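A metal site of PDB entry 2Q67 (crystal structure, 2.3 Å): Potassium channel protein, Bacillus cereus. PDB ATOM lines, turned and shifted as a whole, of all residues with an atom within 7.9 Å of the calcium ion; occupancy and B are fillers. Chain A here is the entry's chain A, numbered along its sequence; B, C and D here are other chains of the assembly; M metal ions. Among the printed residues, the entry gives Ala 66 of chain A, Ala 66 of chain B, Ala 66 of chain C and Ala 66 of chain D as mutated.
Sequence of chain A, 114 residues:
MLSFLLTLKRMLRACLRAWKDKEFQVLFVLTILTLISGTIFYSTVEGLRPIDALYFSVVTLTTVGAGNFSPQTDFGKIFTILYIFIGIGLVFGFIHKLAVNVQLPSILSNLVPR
The backbone carbonyl oxygen of Val 59 of chain A sits at hydrogen-bond distance from the backbone NH of Val 64 of chain A.
The backbone NH of Val 64 of chain B sits at hydrogen-bond distance from the backbone carbonyl oxygen of Val 59 of chain B (3.0 Å).
N of Val 64 of chain C is in hydrogen-bond range of O of Val 59 of chain C (3.0 Å).
O of Thr 63 of chain B binds the calcium ion.
The calcium ion is bound by O of Thr 63 of chain C, at 2.6 Å.
O of Thr 63 of chain D binds the calcium ion (2.6 Å).
O of Thr 63 of chain A binds the calcium ion (2.6 Å).
O of Val 64 of chain D binds the calcium ion.
The backbone carbonyl oxygen (O) of Val 64 of chain A is bound to the calcium ion (2.6 Å).
The backbone carbonyl oxygen (O) of Val 64 of chain B binds the calcium ion, 2.7 Å away.
The backbone carbonyl oxygen (O) of Val 64 of chain C binds the calcium ion, at 2.7 Å.
The calcium ion has eight donor atoms within binding distance.
Of the 24 residues printed, 8 come within 4 Å of the calcium ion.
The nearest printed residue that does not touch the calcium ion is Gly 65 of chain C (4.3 Å).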
ATOM      1  N   VAL A  59      11.259 -26.321 -18.897  1.00  0.00           N
ATOM      2  CA  VAL A  59      10.268 -25.260 -18.855  1.00  0.00           C
ATOM      3  C   VAL A  59      10.884 -23.901 -18.551  1.00  0.00           C
ATOM      4  O   VAL A  59      10.310 -22.858 -18.874  1.00  0.00           O
ATOM      5  CB  VAL A  59       9.131 -25.554 -17.845  1.00  0.00           C
ATOM      6  CG1 VAL A  59       8.486 -26.875 -18.193  1.00  0.00           C
ATOM      7  CG2 VAL A  59       9.671 -25.561 -16.404  1.00  0.00           C
ATOM      8  N   THR A  62      13.022 -22.656 -21.945  1.00  0.00           N
ATOM      9  CA  THR A  62      12.160 -22.366 -23.076  1.00  0.00           C
ATOM     10  C   THR A  62      11.169 -21.216 -22.803  1.00  0.00           C
ATOM     11  O   THR A  62      10.390 -20.850 -23.686  1.00  0.00           O
ATOM     12  CB  THR A  62      11.357 -23.627 -23.461  1.00  0.00           C
ATOM     13  OG1 THR A  62      10.610 -24.080 -22.326  1.00  0.00           O
ATOM     14  CG2 THR A  62      12.307 -24.736 -23.893  1.00  0.00           C
ATOM     15  N   THR A  63      11.247 -20.680 -21.587  1.00  0.00           N
ATOM     16  CA  THR A  63      10.393 -19.584 -21.080  1.00  0.00           C
ATOM     17  C   THR A  63       8.973 -20.052 -20.838  1.00  0.00           C
ATOM     18  O   THR A  63       8.094 -19.234 -20.578  1.00  0.00           O
ATOM     19  CB  THR A  63      10.325 -18.341 -22.009  1.00  0.00           C
ATOM     20  OG1 THR A  63       9.396 -18.567 -23.079  1.00  0.00           O
ATOM     21  CG2 THR A  63      11.688 -17.987 -22.568  1.00  0.00           C
ATOM     22  N   VAL A  64       8.742 -21.352 -20.934  1.00  0.00           N
ATOM     23  CA  VAL A  64       7.404 -21.868 -20.655  1.00  0.00           C
ATOM     24  C   VAL A  64       7.084 -21.501 -19.209  1.00  0.00           C
ATOM     25  O   VAL A  64       6.056 -20.890 -18.929  1.00  0.00           O
ATOM     26  CB  VAL A  64       7.331 -23.420 -20.822  1.00  0.00           C
ATOM     27  CG1 VAL A  64       6.002 -23.949 -20.242  1.00  0.00           C
ATOM     28  CG2 VAL A  64       7.449 -23.798 -22.292  1.00  0.00           C
ATOM     29  N   GLY A  65       7.991 -21.859 -18.297  1.00  0.00           N
ATOM     30  CA  GLY A  65       7.802 -21.560 -16.891  1.00  0.00           C
ATOM     31  C   GLY A  65       7.153 -22.695 -16.126  1.00  0.00           C
ATOM     32  O   GLY A  65       6.243 -23.354 -16.619  1.00  0.00           O
ATOM     33  N   ALA A  66       7.635 -22.928 -14.906  1.00  0.00           N
ATOM     34  CA  ALA A  66       7.121 -23.979 -14.029  1.00  0.00           C
ATOM     35  C   ALA A  66       5.884 -23.518 -13.262  1.00  0.00           C
ATOM     36  O   ALA A  66       5.852 -22.414 -12.725  1.00  0.00           O
ATOM     37  CB  ALA A  66       8.209 -24.411 -13.052  1.00  0.00           C
ATOM     38  N   VAL B  59      -1.483 -23.861 -22.813  1.00  0.00           N
ATOM     39  CA  VAL B  59      -0.528 -22.990 -22.131  1.00  0.00           C
ATOM     40  C   VAL B  59       0.898 -23.534 -22.185  1.00  0.00           C
ATOM     41  O   VAL B  59       1.863 -22.786 -22.033  1.00  0.00           O
ATOM     42  CB  VAL B  59      -0.906 -22.754 -20.661  1.00  0.00           C
ATOM     43  CG1 VAL B  59      -2.210 -22.001 -20.604  1.00  0.00           C
ATOM     44  CG2 VAL B  59      -0.991 -24.073 -19.915  1.00  0.00           C
ATOM     45  N   THR B  62       2.321 -23.130 -26.049  1.00  0.00           N
ATOM     46  CA  THR B  62       2.525 -21.726 -26.386  1.00  0.00           C
ATOM     47  C   THR B  62       3.564 -20.999 -25.532  1.00  0.00           C
ATOM     48  O   THR B  62       3.874 -19.832 -25.797  1.00  0.00           O
ATOM     49  CB  THR B  62       1.198 -20.942 -26.294  1.00  0.00           C
ATOM     50  OG1 THR B  62       0.665 -21.050 -24.963  1.00  0.00           O
ATOM     51  CG2 THR B  62       0.177 -21.502 -27.299  1.00  0.00           C
ATOM     52  N   THR B  63       4.084 -21.691 -24.530  1.00  0.00           N
ATOM     53  CA  THR B  63       5.076 -21.188 -23.555  1.00  0.00           C
ATOM     54  C   THR B  63       4.452 -20.236 -22.563  1.00  0.00           C
ATOM     55  O   THR B  63       5.153 -19.622 -21.760  1.00  0.00           O
ATOM     56  CB  THR B  63       6.289 -20.473 -24.194  1.00  0.00           C
ATOM     57  OG1 THR B  63       5.943 -19.105 -24.458  1.00  0.00           O
ATOM     58  CG2 THR B  63       6.729 -21.172 -25.495  1.00  0.00           C
ATOM     59  N   VAL B  64       3.124 -20.117 -22.615  1.00  0.00           N
ATOM     60  CA  VAL B  64       2.453 -19.273 -21.654  1.00  0.00           C
ATOM     61  C   VAL B  64       2.781 -19.837 -20.267  1.00  0.00           C
ATOM     62  O   VAL B  64       3.232 -19.105 -19.383  1.00  0.00           O
ATOM     63  CB  VAL B  64       0.906 -19.273 -21.862  1.00  0.00           C
ATOM     64  CG1 VAL B  64       0.206 -18.717 -20.628  1.00  0.00           C
ATOM     65  CG2 VAL B  64       0.541 -18.422 -23.078  1.00  0.00           C
ATOM     66  N   GLY B  65       2.560 -21.143 -20.104  1.00  0.00           N
ATOM     67  CA  GLY B  65       2.834 -21.771 -18.825  1.00  0.00           C
ATOM     68  C   GLY B  65       1.606 -21.852 -17.923  1.00  0.00           C
ATOM     69  O   GLY B  65       0.779 -20.941 -17.915  1.00  0.00           O
ATOM     70  N   ALA B  66       1.495 -22.958 -17.183  1.00  0.00           N
ATOM     71  CA  ALA B  66       0.375 -23.212 -16.265  1.00  0.00           C
ATOM     72  C   ALA B  66       0.658 -22.638 -14.893  1.00  0.00           C
ATOM     73  O   ALA B  66       1.769 -22.752 -14.383  1.00  0.00           O
ATOM     74  CB  ALA B  66       0.126 -24.699 -16.152  1.00  0.00           C
ATOM     75  N   VAL C  59      12.302 -13.587 -14.232  1.00  0.00           N
ATOM     76  CA  VAL C  59      11.327 -14.476 -14.860  1.00  0.00           C
ATOM     77  C   VAL C  59      10.141 -13.717 -15.450  1.00  0.00           C
ATOM     78  O   VAL C  59       9.450 -14.219 -16.335  1.00  0.00           O
ATOM     79  CB  VAL C  59      10.792 -15.533 -13.881  1.00  0.00           C
ATOM     80  CG1 VAL C  59      11.931 -16.446 -13.471  1.00  0.00           C
ATOM     81  CG2 VAL C  59      10.150 -14.867 -12.678  1.00  0.00           C
ATOM     82  N   THR C  62      11.419 -11.696 -18.827  1.00  0.00           N
ATOM     83  CA  THR C  62      11.741 -12.627 -19.902  1.00  0.00           C
ATOM     84  C   THR C  62      10.577 -13.478 -20.398  1.00  0.00           C
ATOM     85  O   THR C  62      10.719 -14.227 -21.367  1.00  0.00           O
ATOM     86  CB  THR C  62      12.875 -13.584 -19.475  1.00  0.00           C
ATOM     87  OG1 THR C  62      12.474 -14.314 -18.304  1.00  0.00           O
ATOM     88  CG2 THR C  62      14.156 -12.790 -19.168  1.00  0.00           C
ATOM     89  N   THR C  63       9.429 -13.338 -19.738  1.00  0.00           N
ATOM     90  CA  THR C  63       8.177 -14.074 -20.016  1.00  0.00           C
ATOM     91  C   THR C  63       8.261 -15.511 -19.560  1.00  0.00           C
ATOM     92  O   THR C  63       7.360 -16.305 -19.826  1.00  0.00           O
ATOM     93  CB  THR C  63       7.765 -14.082 -21.503  1.00  0.00           C
ATOM     94  OG1 THR C  63       8.456 -15.128 -22.188  1.00  0.00           O
ATOM     95  CG2 THR C  63       8.050 -12.719 -22.171  1.00  0.00           C
ATOM     96  N   VAL C  64       9.341 -15.841 -18.865  1.00  0.00           N
ATOM     97  CA  VAL C  64       9.467 -17.187 -18.340  1.00  0.00           C
ATOM     98  C   VAL C  64       8.281 -17.406 -17.402  1.00  0.00           C
ATOM     99  O   VAL C  64       7.541 -18.386 -17.536  1.00  0.00           O
ATOM    100  CB  VAL C  64      10.793 -17.385 -17.543  1.00  0.00           C
ATOM    101  CG1 VAL C  64      10.713 -18.642 -16.685  1.00  0.00           C
ATOM    102  CG2 VAL C  64      11.972 -17.505 -18.508  1.00  0.00           C
ATOM    103  N   GLY C  65       8.082 -16.470 -16.480  1.00  0.00           N
ATOM    104  CA  GLY C  65       6.986 -16.576 -15.537  1.00  0.00           C
ATOM    105  C   GLY C  65       7.387 -17.237 -14.222  1.00  0.00           C
ATOM    106  O   GLY C  65       8.207 -18.154 -14.212  1.00  0.00           O
ATOM    107  N   ALA C  66       6.811 -16.748 -13.121  1.00  0.00           N
ATOM    108  CA  ALA C  66       7.085 -17.255 -11.768  1.00  0.00           C
ATOM    109  C   ALA C  66       6.157 -18.412 -11.428  1.00  0.00           C
ATOM    110  O   ALA C  66       4.962 -18.357 -11.720  1.00  0.00           O
ATOM    111  CB  ALA C  66       6.914 -16.145 -10.755  1.00  0.00           C
ATOM    112  N   VAL D  59      -0.433 -11.121 -18.165  1.00  0.00           N
ATOM    113  CA  VAL D  59       0.525 -12.213 -18.118  1.00  0.00           C
ATOM    114  C   VAL D  59       0.136 -13.368 -19.030  1.00  0.00           C
ATOM    115  O   VAL D  59       0.983 -14.166 -19.440  1.00  0.00           O
ATOM    116  CB  VAL D  59       0.748 -12.739 -16.678  1.00  0.00           C
ATOM    117  CG1 VAL D  59       1.193 -11.597 -15.794  1.00  0.00           C
ATOM    118  CG2 VAL D  59      -0.532 -13.397 -16.134  1.00  0.00           C
ATOM    119  N   THR D  62       0.744 -12.146 -23.003  1.00  0.00           N
ATOM    120  CA  THR D  62       2.155 -11.955 -23.319  1.00  0.00           C
ATOM    121  C   THR D  62       2.984 -13.238 -23.182  1.00  0.00           C
ATOM    122  O   THR D  62       4.190 -13.221 -23.442  1.00  0.00           O
ATOM    123  CB  THR D  62       2.749 -10.869 -22.398  1.00  0.00           C
ATOM    124  OG1 THR D  62       2.563 -11.254 -21.030  1.00  0.00           O
ATOM    125  CG2 THR D  62       2.046  -9.538 -22.628  1.00  0.00           C
ATOM    126  N   THR D  63       2.306 -14.313 -22.788  1.00  0.00           N
ATOM    127  CA  THR D  63       2.886 -15.654 -22.562  1.00  0.00           C
ATOM    128  C   THR D  63       3.753 -15.684 -21.321  1.00  0.00           C
ATOM    129  O   THR D  63       4.445 -16.670 -21.080  1.00  0.00           O
ATOM    130  CB  THR D  63       3.749 -16.196 -23.742  1.00  0.00           C
ATOM    131  OG1 THR D  63       5.057 -15.618 -23.710  1.00  0.00           O
ATOM    132  CG2 THR D  63       3.085 -15.910 -25.079  1.00  0.00           C
ATOM    133  N   VAL D  64       3.731 -14.611 -20.544  1.00  0.00           N
ATOM    134  CA  VAL D  64       4.502 -14.604 -19.304  1.00  0.00           C
ATOM    135  C   VAL D  64       3.954 -15.739 -18.445  1.00  0.00           C
ATOM    136  O   VAL D  64       4.717 -16.600 -17.991  1.00  0.00           O
ATOM    137  CB  VAL D  64       4.349 -13.256 -18.529  1.00  0.00           C
ATOM    138  CG1 VAL D  64       4.930 -13.397 -17.107  1.00  0.00           C
ATOM    139  CG2 VAL D  64       5.057 -12.135 -19.277  1.00  0.00           C
ATOM    140  N   GLY D  65       2.641 -15.757 -18.247  1.00  0.00           N
ATOM    141  CA  GLY D  65       2.010 -16.792 -17.454  1.00  0.00           C
ATOM    142  C   GLY D  65       1.833 -16.400 -16.002  1.00  0.00           C
ATOM    143  O   GLY D  65       2.703 -15.777 -15.401  1.00  0.00           O
ATOM    144  N   ALA D  66       0.685 -16.766 -15.434  1.00  0.00           N
ATOM    145  CA  ALA D  66       0.352 -16.476 -14.040  1.00  0.00           C
ATOM    146  C   ALA D  66       0.949 -17.512 -13.091  1.00  0.00           C
ATOM    147  O   ALA D  66       0.874 -18.712 -13.341  1.00  0.00           O
ATOM    148  CB  ALA D  66      -1.163 -16.427 -13.872  1.00  0.00           C
HETATM  149 CA    CA M   1       5.812 -18.356 -19.614  1.00  0.00          CA
